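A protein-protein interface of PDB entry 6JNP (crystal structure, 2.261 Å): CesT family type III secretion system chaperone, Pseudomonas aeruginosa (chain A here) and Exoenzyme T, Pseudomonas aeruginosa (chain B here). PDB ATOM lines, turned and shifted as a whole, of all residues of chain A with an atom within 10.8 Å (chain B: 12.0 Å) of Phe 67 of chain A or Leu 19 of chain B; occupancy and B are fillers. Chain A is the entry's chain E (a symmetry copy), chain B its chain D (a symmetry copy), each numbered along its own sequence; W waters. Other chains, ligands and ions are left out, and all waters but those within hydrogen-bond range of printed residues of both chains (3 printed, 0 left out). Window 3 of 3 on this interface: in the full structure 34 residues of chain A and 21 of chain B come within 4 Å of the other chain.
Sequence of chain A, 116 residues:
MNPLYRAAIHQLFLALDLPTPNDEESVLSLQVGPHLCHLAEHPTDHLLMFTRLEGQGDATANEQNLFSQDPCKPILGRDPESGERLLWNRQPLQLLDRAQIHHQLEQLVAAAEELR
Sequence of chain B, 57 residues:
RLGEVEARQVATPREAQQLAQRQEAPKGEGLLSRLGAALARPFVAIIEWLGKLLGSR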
ATOM      1  N   ASN A  62     -36.288 -27.072 -19.391  1.00  0.00           N
ATOM      2  CA  ASN A  62     -35.586 -28.018 -18.538  1.00  0.00           C
ATOM      3  C   ASN A  62     -34.686 -27.261 -17.571  1.00  0.00           C
ATOM      4  O   ASN A  62     -34.326 -26.104 -17.800  1.00  0.00           O
ATOM      5  CB  ASN A  62     -34.766 -29.012 -19.375  1.00  0.00           C
ATOM      6  CG  ASN A  62     -34.109 -30.089 -18.533  1.00  0.00           C
ATOM      7  OD1 ASN A  62     -34.502 -30.329 -17.391  1.00  0.00           O
ATOM      8  ND2 ASN A  62     -33.099 -30.746 -19.095  1.00  0.00           N
ATOM      9  N   GLU A  63     -34.332 -27.941 -16.476  1.00  0.00           N
ATOM     10  CA  GLU A  63     -33.371 -27.409 -15.516  1.00  0.00           C
ATOM     11  C   GLU A  63     -32.019 -27.112 -16.156  1.00  0.00           C
ATOM     12  O   GLU A  63     -31.265 -26.282 -15.635  1.00  0.00           O
ATOM     13  CB  GLU A  63     -33.206 -28.406 -14.361  1.00  0.00           C
ATOM     14  CG  GLU A  63     -32.169 -28.030 -13.310  1.00  0.00           C
ATOM     15  CD  GLU A  63     -32.664 -26.973 -12.343  1.00  0.00           C
ATOM     16  OE1 GLU A  63     -33.821 -27.082 -11.883  1.00  0.00           O
ATOM     17  OE2 GLU A  63     -31.896 -26.036 -12.043  1.00  0.00           O
ATOM     18  N   GLN A  64     -31.709 -27.755 -17.285  1.00  0.00           N
ATOM     19  CA  GLN A  64     -30.394 -27.600 -17.902  1.00  0.00           C
ATOM     20  C   GLN A  64     -30.130 -26.154 -18.310  1.00  0.00           C
ATOM     21  O   GLN A  64     -29.000 -25.667 -18.196  1.00  0.00           O
ATOM     22  CB  GLN A  64     -30.278 -28.526 -19.113  1.00  0.00           C
ATOM     23  CG  GLN A  64     -28.894 -28.560 -19.736  1.00  0.00           C
ATOM     24  CD  GLN A  64     -27.849 -29.118 -18.791  1.00  0.00           C
ATOM     25  OE1 GLN A  64     -28.033 -30.186 -18.206  1.00  0.00           O
ATOM     26  NE2 GLN A  64     -26.747 -28.393 -18.631  1.00  0.00           N
ATOM     27  N   ASN A  65     -31.158 -25.452 -18.786  1.00  0.00           N
ATOM     28  CA  ASN A  65     -31.004 -24.099 -19.301  1.00  0.00           C
ATOM     29  C   ASN A  65     -31.193 -23.032 -18.229  1.00  0.00           C
ATOM     30  O   ASN A  65     -31.481 -21.875 -18.560  1.00  0.00           O
ATOM     31  CB  ASN A  65     -31.972 -23.869 -20.461  1.00  0.00           C
ATOM     32  CG  ASN A  65     -31.702 -24.798 -21.626  1.00  0.00           C
ATOM     33  OD1 ASN A  65     -30.579 -25.268 -21.806  1.00  0.00           O
ATOM     34  ND2 ASN A  65     -32.730 -25.072 -22.418  1.00  0.00           N
ATOM     35  N   LEU A  66     -31.035 -23.394 -16.961  1.00  0.00           N
ATOM     36  CA  LEU A  66     -31.043 -22.439 -15.863  1.00  0.00           C
ATOM     37  C   LEU A  66     -29.608 -22.144 -15.447  1.00  0.00           C
ATOM     38  O   LEU A  66     -28.778 -23.053 -15.363  1.00  0.00           O
ATOM     39  CB  LEU A  66     -31.837 -22.986 -14.678  1.00  0.00           C
ATOM     40  CG  LEU A  66     -31.916 -22.112 -13.428  1.00  0.00           C
ATOM     41  CD1 LEU A  66     -32.483 -20.742 -13.764  1.00  0.00           C
ATOM     42  CD2 LEU A  66     -32.759 -22.800 -12.374  1.00  0.00           C
ATOM     43  N   PHE A  67     -29.316 -20.871 -15.196  1.00  0.00           N
ATOM     44  CA  PHE A  67     -27.951 -20.482 -14.872  1.00  0.00           C
ATOM     45  C   PHE A  67     -27.546 -21.018 -13.505  1.00  0.00           C
ATOM     46  O   PHE A  67     -28.353 -21.068 -12.572  1.00  0.00           O
ATOM     47  CB  PHE A  67     -27.791 -18.958 -14.912  1.00  0.00           C
ATOM     48  CG  PHE A  67     -28.640 -18.221 -13.909  1.00  0.00           C
ATOM     49  CD1 PHE A  67     -28.192 -18.014 -12.613  1.00  0.00           C
ATOM     50  CD2 PHE A  67     -29.876 -17.713 -14.271  1.00  0.00           C
ATOM     51  CE1 PHE A  67     -28.969 -17.337 -11.693  1.00  0.00           C
ATOM     52  CE2 PHE A  67     -30.656 -17.029 -13.355  1.00  0.00           C
ATOM     53  CZ  PHE A  67     -30.200 -16.840 -12.065  1.00  0.00           C
ATOM     54  N   SER A  68     -26.287 -21.435 -13.396  1.00  0.00           N
ATOM     55  CA  SER A  68     -25.709 -21.805 -12.113  1.00  0.00           C
ATOM     56  C   SER A  68     -24.527 -20.894 -11.819  1.00  0.00           C
ATOM     57  O   SER A  68     -24.409 -19.815 -12.409  1.00  0.00           O
ATOM     58  CB  SER A  68     -25.279 -23.274 -12.108  1.00  0.00           C
ATOM     59  OG  SER A  68     -24.162 -23.480 -12.956  1.00  0.00           O
ATOM     60  N   GLN A  69     -23.644 -21.312 -10.915  1.00  0.00           N
ATOM     61  CA  GLN A  69     -22.436 -20.543 -10.648  1.00  0.00           C
ATOM     62  C   GLN A  69     -21.318 -20.853 -11.634  1.00  0.00           C
ATOM     63  O   GLN A  69     -20.301 -20.153 -11.633  1.00  0.00           O
ATOM     64  CB  GLN A  69     -21.948 -20.796  -9.218  1.00  0.00           C
ATOM     65  CG  GLN A  69     -21.122 -22.065  -9.043  1.00  0.00           C
ATOM     66  CD  GLN A  69     -21.932 -23.335  -9.222  1.00  0.00           C
ATOM     67  OE1 GLN A  69     -23.163 -23.304  -9.246  1.00  0.00           O
ATOM     68  NE2 GLN A  69     -21.241 -24.461  -9.346  1.00  0.00           N
ATOM     69  N   ASP A  70     -21.483 -21.880 -12.468  1.00  0.00           N
ATOM     70  CA  ASP A  70     -20.471 -22.251 -13.442  1.00  0.00           C
ATOM     71  C   ASP A  70     -20.876 -21.717 -14.806  1.00  0.00           C
ATOM     72  O   ASP A  70     -21.852 -22.217 -15.389  1.00  0.00           O
ATOM     73  CB  ASP A  70     -20.306 -23.770 -13.491  1.00  0.00           C
ATOM     74  CG  ASP A  70     -19.037 -24.201 -14.207  1.00  0.00           C
ATOM     75  OD1 ASP A  70     -18.469 -23.394 -14.970  1.00  0.00           O
ATOM     76  OD2 ASP A  70     -18.608 -25.357 -14.004  1.00  0.00           O
ATOM     77  N   PRO A  71     -20.178 -20.721 -15.355  1.00  0.00           N
ATOM     78  CA  PRO A  71     -20.514 -20.249 -16.708  1.00  0.00           C
ATOM     79  C   PRO A  71     -20.343 -21.314 -17.775  1.00  0.00           C
ATOM     80  O   PRO A  71     -20.959 -21.207 -18.844  1.00  0.00           O
ATOM     81  CB  PRO A  71     -19.545 -19.078 -16.927  1.00  0.00           C
ATOM     82  CG  PRO A  71     -19.091 -18.683 -15.552  1.00  0.00           C
ATOM     83  CD  PRO A  71     -19.077 -19.951 -14.757  1.00  0.00           C
ATOM     84  N   CYS A  72     -19.530 -22.338 -17.521  1.00  0.00           N
ATOM     85  CA  CYS A  72     -19.352 -23.438 -18.458  1.00  0.00           C
ATOM     86  C   CYS A  72     -20.510 -24.426 -18.444  1.00  0.00           C
ATOM     87  O   CYS A  72     -20.492 -25.379 -19.232  1.00  0.00           O
ATOM     88  CB  CYS A  72     -18.046 -24.179 -18.162  1.00  0.00           C
ATOM     89  SG  CYS A  72     -16.563 -23.247 -18.585  1.00  0.00           S
ATOM     90  N   LYS A  73     -21.498 -24.235 -17.576  1.00  0.00           N
ATOM     91  CA  LYS A  73     -22.677 -25.087 -17.601  1.00  0.00           C
ATOM     92  C   LYS A  73     -23.368 -24.927 -18.948  1.00  0.00           C
ATOM     93  O   LYS A  73     -23.789 -23.812 -19.291  1.00  0.00           O
ATOM     94  CB  LYS A  73     -23.645 -24.746 -16.472  1.00  0.00           C
ATOM     95  CG  LYS A  73     -24.812 -25.720 -16.386  1.00  0.00           C
ATOM     96  CD  LYS A  73     -25.967 -25.180 -15.560  1.00  0.00           C
ATOM     97  CE  LYS A  73     -27.144 -26.147 -15.593  1.00  0.00           C
ATOM     98  NZ  LYS A  73     -28.345 -25.615 -14.890  1.00  0.00           N
ATOM     99  N   PRO A  74     -23.497 -25.986 -19.738  1.00  0.00           N
ATOM    100  CA  PRO A  74     -23.998 -25.833 -21.104  1.00  0.00           C
ATOM    101  C   PRO A  74     -25.506 -25.639 -21.161  1.00  0.00           C
ATOM    102  O   PRO A  74     -26.251 -25.941 -20.227  1.00  0.00           O
ATOM    103  CB  PRO A  74     -23.588 -27.145 -21.780  1.00  0.00           C
ATOM    104  CG  PRO A  74     -23.520 -28.116 -20.677  1.00  0.00           C
ATOM    105  CD  PRO A  74     -23.074 -27.367 -19.454  1.00  0.00           C
ATOM    106  N   ILE A  75     -25.932 -25.109 -22.298  1.00  0.00           N
ATOM    107  CA  ILE A  75     -27.324 -24.855 -22.632  1.00  0.00           C
ATOM    108  C   ILE A  75     -27.803 -25.975 -23.539  1.00  0.00           C
ATOM    109  O   ILE A  75     -27.050 -26.466 -24.393  1.00  0.00           O
ATOM    110  CB  ILE A  75     -27.473 -23.485 -23.321  1.00  0.00           C
ATOM    111  CG1 ILE A  75     -26.777 -22.394 -22.502  1.00  0.00           C
ATOM    112  CG2 ILE A  75     -28.936 -23.149 -23.567  1.00  0.00           C
ATOM    113  CD1 ILE A  75     -27.275 -22.283 -21.082  1.00  0.00           C
ATOM    114  N   LEU A  76     -29.055 -26.387 -23.351  1.00  0.00           N
ATOM    115  CA  LEU A  76     -29.700 -27.379 -24.205  1.00  0.00           C
ATOM    116  C   LEU A  76     -30.660 -26.639 -25.130  1.00  0.00           C
ATOM    117  O   LEU A  76     -31.743 -26.216 -24.713  1.00  0.00           O
ATOM    118  CB  LEU A  76     -30.423 -28.431 -23.369  1.00  0.00           C
ATOM    119  CG  LEU A  76     -31.245 -29.457 -24.153  1.00  0.00           C
ATOM    120  CD1 LEU A  76     -30.407 -30.088 -25.249  1.00  0.00           C
ATOM    121  CD2 LEU A  76     -31.800 -30.525 -23.227  1.00  0.00           C
ATOM    122  N   THR B  12     -35.158  -4.810  -5.311  1.00  0.00           N
ATOM    123  CA  THR B  12     -34.928  -6.177  -5.746  1.00  0.00           C
ATOM    124  C   THR B  12     -35.719  -7.130  -4.868  1.00  0.00           C
ATOM    125  O   THR B  12     -35.505  -7.147  -3.645  1.00  0.00           O
ATOM    126  CB  THR B  12     -33.443  -6.517  -5.684  1.00  0.00           C
ATOM    127  OG1 THR B  12     -32.703  -5.572  -6.469  1.00  0.00           O
ATOM    128  CG2 THR B  12     -33.199  -7.918  -6.223  1.00  0.00           C
ATOM    129  N   PRO B  13     -36.634  -7.921  -5.425  1.00  0.00           N
ATOM    130  CA  PRO B  13     -37.331  -8.924  -4.612  1.00  0.00           C
ATOM    131  C   PRO B  13     -36.354  -9.944  -4.048  1.00  0.00           C
ATOM    132  O   PRO B  13     -35.382 -10.327  -4.701  1.00  0.00           O
ATOM    133  CB  PRO B  13     -38.312  -9.565  -5.602  1.00  0.00           C
ATOM    134  CG  PRO B  13     -38.493  -8.538  -6.676  1.00  0.00           C
ATOM    135  CD  PRO B  13     -37.168  -7.847  -6.796  1.00  0.00           C
ATOM    136  N   ARG B  14     -36.621 -10.380  -2.813  1.00  0.00           N
ATOM    137  CA  ARG B  14     -35.723 -11.316  -2.146  1.00  0.00           C
ATOM    138  C   ARG B  14     -35.669 -12.654  -2.869  1.00  0.00           C
ATOM    139  O   ARG B  14     -34.633 -13.329  -2.844  1.00  0.00           O
ATOM    140  CB  ARG B  14     -36.154 -11.514  -0.692  1.00  0.00           C
ATOM    141  CG  ARG B  14     -36.329 -10.216   0.079  1.00  0.00           C
ATOM    142  CD  ARG B  14     -37.734 -10.110   0.647  1.00  0.00           C
ATOM    143  NE  ARG B  14     -38.724 -10.643  -0.282  1.00  0.00           N
ATOM    144  CZ  ARG B  14     -39.228  -9.966  -1.309  1.00  0.00           C
ATOM    145  NH1 ARG B  14     -38.831  -8.722  -1.546  1.00  0.00           N
ATOM    146  NH2 ARG B  14     -40.122 -10.537  -2.105  1.00  0.00           N
ATOM    147  N   GLU B  15     -36.765 -13.055  -3.516  1.00  0.00           N
ATOM    148  CA  GLU B  15     -36.728 -14.255  -4.344  1.00  0.00           C
ATOM    149  C   GLU B  15     -35.760 -14.080  -5.507  1.00  0.00           C
ATOM    150  O   GLU B  15     -35.037 -15.015  -5.873  1.00  0.00           O
ATOM    151  CB  GLU B  15     -38.135 -14.595  -4.840  1.00  0.00           C
ATOM    152  CG  GLU B  15     -38.895 -13.428  -5.463  1.00  0.00           C
ATOM    153  CD  GLU B  15     -38.606 -13.258  -6.943  1.00  0.00           C
ATOM    154  OE1 GLU B  15     -37.969 -14.156  -7.529  1.00  0.00           O
ATOM    155  OE2 GLU B  15     -39.012 -12.226  -7.519  1.00  0.00           O
ATOM    156  N   ALA B  16     -35.711 -12.877  -6.083  1.00  0.00           N
ATOM    157  CA  ALA B  16     -34.764 -12.612  -7.160  1.00  0.00           C
ATOM    158  C   ALA B  16     -33.331 -12.609  -6.643  1.00  0.00           C
ATOM    159  O   ALA B  16     -32.421 -13.091  -7.325  1.00  0.00           O
ATOM    160  CB  ALA B  16     -35.096 -11.284  -7.838  1.00  0.00           C
ATOM    161  N   GLN B  17     -33.110 -12.075  -5.438  1.00  0.00           N
ATOM    162  CA  GLN B  17     -31.774 -12.107  -4.854  1.00  0.00           C
ATOM    163  C   GLN B  17     -31.339 -13.532  -4.530  1.00  0.00           C
ATOM    164  O   GLN B  17     -30.146 -13.848  -4.609  1.00  0.00           O
ATOM    165  CB  GLN B  17     -31.725 -11.231  -3.601  1.00  0.00           C
ATOM    166  CG  GLN B  17     -30.337 -11.109  -2.987  1.00  0.00           C
ATOM    167  CD  GLN B  17     -30.218  -9.938  -2.030  1.00  0.00           C
ATOM    168  OE1 GLN B  17     -31.219  -9.358  -1.610  1.00  0.00           O
ATOM    169  NE2 GLN B  17     -28.985  -9.580  -1.687  1.00  0.00           N
ATOM    170  N   GLN B  18     -32.286 -14.400  -4.166  1.00  0.00           N
ATOM    171  CA  GLN B  18     -31.957 -15.806  -3.949  1.00  0.00           C
ATOM    172  C   GLN B  18     -31.655 -16.510  -5.265  1.00  0.00           C
ATOM    173  O   GLN B  18     -30.724 -17.320  -5.343  1.00  0.00           O
ATOM    174  CB  GLN B  18     -33.103 -16.506  -3.218  1.00  0.00           C
ATOM    175  CG  GLN B  18     -33.122 -16.262  -1.720  1.00  0.00           C
ATOM    176  CD  GLN B  18     -32.034 -17.028  -0.996  1.00  0.00           C
ATOM    177  OE1 GLN B  18     -31.652 -18.123  -1.408  1.00  0.00           O
ATOM    178  NE2 GLN B  18     -31.524 -16.452   0.087  1.00  0.00           N
ATOM    179  N   LEU B  19     -32.433 -16.214  -6.309  1.00  0.00           N
ATOM    180  CA  LEU B  19     -32.190 -16.823  -7.613  1.00  0.00           C
ATOM    181  C   LEU B  19     -30.853 -16.377  -8.192  1.00  0.00           C
ATOM    182  O   LEU B  19     -30.157 -17.167  -8.840  1.00  0.00           O
ATOM    183  CB  LEU B  19     -33.330 -16.475  -8.570  1.00  0.00           C
ATOM    184  CG  LEU B  19     -33.944 -17.611  -9.390  1.00  0.00           C
ATOM    185  CD1 LEU B  19     -34.933 -17.049 -10.391  1.00  0.00           C
ATOM    186  CD2 LEU B  19     -32.879 -18.435 -10.093  1.00  0.00           C
ATOM    187  N   ALA B  20     -30.475 -15.117  -7.964  1.00  0.00           N
ATOM    188  CA  ALA B  20     -29.254 -14.562  -8.534  1.00  0.00           C
ATOM    189  C   ALA B  20     -27.989 -15.185  -7.963  1.00  0.00           C
ATOM    190  O   ALA B  20     -26.896 -14.878  -8.452  1.00  0.00           O
ATOM    191  CB  ALA B  20     -29.218 -13.049  -8.317  1.00  0.00           C
ATOM    192  N   GLN B  21     -28.101 -16.040  -6.944  1.00  0.00           N
ATOM    193  CA  GLN B  21     -26.935 -16.673  -6.343  1.00  0.00           C
ATOM    194  C   GLN B  21     -27.084 -18.189  -6.268  1.00  0.00           C
ATOM    195  O   GLN B  21     -26.343 -18.838  -5.521  1.00  0.00           O
ATOM    196  CB  GLN B  21     -26.670 -16.100  -4.949  1.00  0.00           C
ATOM    197  CG  GLN B  21     -27.822 -16.285  -3.977  1.00  0.00           C
ATOM    198  CD  GLN B  21     -27.495 -15.787  -2.584  1.00  0.00           C
ATOM    199  OE1 GLN B  21     -26.408 -15.266  -2.339  1.00  0.00           O
ATOM    200  NE2 GLN B  21     -28.437 -15.949  -1.663  1.00  0.00           N
ATOM    201  N   ARG B  22     -28.019 -18.767  -7.021  1.00  0.00           N
ATOM    202  CA  ARG B  22     -28.235 -20.205  -6.955  1.00  0.00           C
ATOM    203  C   ARG B  22     -26.997 -20.952  -7.436  1.00  0.00           C
ATOM    204  O   ARG B  22     -26.281 -20.506  -8.336  1.00  0.00           O
ATOM    205  CB  ARG B  22     -29.454 -20.610  -7.785  1.00  0.00           C
ATOM    206  CG  ARG B  22     -29.258 -20.525  -9.287  1.00  0.00           C
ATOM    207  CD  ARG B  22     -30.431 -21.153 -10.024  1.00  0.00           C
ATOM    208  NE  ARG B  22     -30.592 -22.568  -9.700  1.00  0.00           N
ATOM    209  CZ  ARG B  22     -30.049 -23.562 -10.397  1.00  0.00           C
ATOM    210  NH1 ARG B  22     -29.309 -23.300 -11.465  1.00  0.00           N
ATOM    211  NH2 ARG B  22     -30.250 -24.820 -10.029  1.00  0.00           N
ATOM    212  N   GLN B  23     -26.739 -22.096  -6.810  1.00  0.00           N
ATOM    213  CA  GLN B  23     -25.564 -22.896  -7.108  1.00  0.00           C
ATOM    214  C   GLN B  23     -25.971 -24.340  -7.351  1.00  0.00           C
ATOM    215  O   GLN B  23     -27.024 -24.799  -6.900  1.00  0.00           O
ATOM    216  CB  GLN B  23     -24.530 -22.831  -5.977  1.00  0.00           C
ATOM    217  CG  GLN B  23     -23.859 -21.480  -5.826  1.00  0.00           C
ATOM    218  CD  GLN B  23     -22.748 -21.496  -4.797  1.00  0.00           C
ATOM    219  OE1 GLN B  23     -22.754 -22.308  -3.872  1.00  0.00           O
ATOM    220  NE2 GLN B  23     -21.782 -20.599  -4.958  1.00  0.00           N
ATOM    221  N   GLU B  24     -25.116 -25.049  -8.080  1.00  0.00           N
ATOM    222  CA  GLU B  24     -25.280 -26.470  -8.331  1.00  0.00           C
ATOM    223  C   GLU B  24     -23.999 -27.187  -7.935  1.00  0.00           C
ATOM    224  O   GLU B  24     -22.907 -26.614  -7.988  1.00  0.00           O
ATOM    225  CB  GLU B  24     -25.607 -26.755  -9.803  1.00  0.00           C
ATOM    226  CG  GLU B  24     -26.880 -26.088 -10.295  1.00  0.00           C
ATOM    227  CD  GLU B  24     -27.160 -26.378 -11.758  1.00  0.00           C
ATOM    228  OE1 GLU B  24     -26.326 -27.045 -12.405  1.00  0.00           O
ATOM    229  OE2 GLU B  24     -28.216 -25.940 -12.257  1.00  0.00           O
ATOM    230  N   ALA B  25     -24.145 -28.442  -7.528  1.00  0.00           N
ATOM    231  CA  ALA B  25     -22.983 -29.228  -7.152  1.00  0.00           C
ATOM    232  C   ALA B  25     -22.087 -29.445  -8.366  1.00  0.00           C
ATOM    233  O   ALA B  25     -22.586 -29.622  -9.484  1.00  0.00           O
ATOM    234  CB  ALA B  25     -23.409 -30.573  -6.565  1.00  0.00           C
ATOM    235  N   LYS B  27     -20.083 -31.210 -11.185  1.00  0.00           N
ATOM    236  CA  LYS B  27     -20.350 -32.466 -11.866  1.00  0.00           C
ATOM    237  C   LYS B  27     -19.224 -32.773 -12.844  1.00  0.00           C
ATOM    238  O   LYS B  27     -18.503 -31.880 -13.299  1.00  0.00           O
ATOM    239  CB  LYS B  27     -21.695 -32.429 -12.606  1.00  0.00           C
ATOM    240  CG  LYS B  27     -22.010 -31.087 -13.245  1.00  0.00           C
ATOM    241  CD  LYS B  27     -23.131 -31.206 -14.264  1.00  0.00           C
ATOM    242  CE  LYS B  27     -24.379 -31.830 -13.663  1.00  0.00           C
ATOM    243  NZ  LYS B  27     -25.457 -31.977 -14.681  1.00  0.00           N
HETATM  244  O   HOH W   1     -24.891 -29.243 -16.669  1.00  0.00           O
HETATM  245  O   HOH W   2     -23.202 -25.807 -12.729  1.00  0.00           O
HETATM  246  O   HOH W   3     -21.483 -26.648 -10.760  1.00  0.00           O
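The guanidinium group (NH2) of Arg 22 of chain B lies within salt-bridge range of the side-chain carboxylate (OE2) of Glu 63 of chain A (2.9 Å). O of Phe 67 of chain A sits at hydrogen-bond distance from NH1 of Arg 22 of chain B (2.7 Å). N of Glu 24 of chain B sits at hydrogen-bond distance from OE1 of Gln 69 of chain A, at 2.9 Å. The side-chain carboxylate (OE2) of Glu 24 of chain B lies within salt-bridge range of the side-chain amino group (NZ) of Lys 73 of chain A (2.7 Å).
NH1 of Arg 22 of chain B is in salt-bridge range of OE2 of Glu 24 of chain B (3.0 Å). NZ of Lys 73 of chain A sits at hydrogen-bond distance from O of Glu 63 of chain A, at 3.1 Å. O of Gln 64 of chain A sits close to NZ of Lys 73 of chain A (3.4 Å). The side-chain amino group (NZ) of Lys 73 of chain A lies within hydrogen-bond range of the backbone carbonyl oxygen (O) of Leu 66 of chain A (2.6 Å). OG of Ser 68 of chain A lies within hydrogen-bond range of N of Asp 70 of chain A, 3.2 Å away.
Among the printed residues, merely in contact across the chains: Phe 67 of chain A with Leu 19 of chain B (3.1 Å), Gln 69 of chain A with Gln 23 of chain B (3.2 Å), Leu 66 of chain A with Arg 22 of chain B (3.4 Å), Ser 68 of chain A with Glu 24 of chain B (3.6 Å), Glu 63 of chain A with Glu 24 of chain B (3.7 Å), Gln 69 of chain A with Arg 22 of chain B (3.8 Å) and Ser 68 of chain A with Arg 22 of chain B (3.9 Å).
Asn 62 of chain A touches none of the printed residues of chain B. Of the printed residues of chain B, Glu 63 of chain A touches Arg 22 and Glu 24. Phe 67 of chain A touches just these residues of chain B: Leu 19 and Arg 22. Of chain B, only Arg 22 and Glu 24 come within 4 Å of Ser 68 of chain A. Of the printed residues of chain B, Gln 69 of chain A touches Arg 22, Gln 23 and Glu 24. Lys 73 of chain A touches just one residue of chain B: Glu 24. Ala 16 of chain B touches none of the printed residues of chain A. Of chain A, only Phe 67 (3.1 Å) comes within 4 Å of Leu 19 of chain B. Arg 22 of chain B touches just these residues of chain A: Glu 63 (2.9 Å), Leu 66 (3.4 Å), Phe 67 (2.7 Å), Ser 68 (3.9 Å) and Gln 69 (3.8 Å). Printed residues of chain A within 4 Å of Gln 23 of chain B: Gln 69 (3.2 Å). Of the printed residues of chain A, Glu 24 of chain B touches Glu 63, Ser 68, Gln 69 and Lys 73. The nearest printed residue of chain B that does not touch Gln 69 of chain A is Ala 25 of chain B (5.1 Å).
Printed residues of chain A that touch a printed residue of chain B: Glu 63, Leu 66, Phe 67, Ser 68, Gln 69 and Lys 73. Of the 15 printed residues of chain B, 4 touch a printed residue of chain A. Hydrophobic or aromatic side chains of chain B within 4 Å of the printed part of chain A: Leu 19. Among the printed residues, 11 pairs touch across the chains.
Water W2 bridges the side-chain hydroxyl of Ser 68 of chain A (2.5 Å) and the side-chain carboxylate of Glu 24 of chain B (3.4 Å). Water W3 lies within hydrogen-bond range of NE2 of Gln 69 of chain A (2.6 Å), O of Glu 24 of chain B (3.1 Å) and O of Ala 25 of chain B (3.4 Å). Water W1 bridges the side-chain amide nitrogen of Gln 64 of chain A (2.8 Å) and the side-chain amino group of Lys 27 of chain B (3.4 Å).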
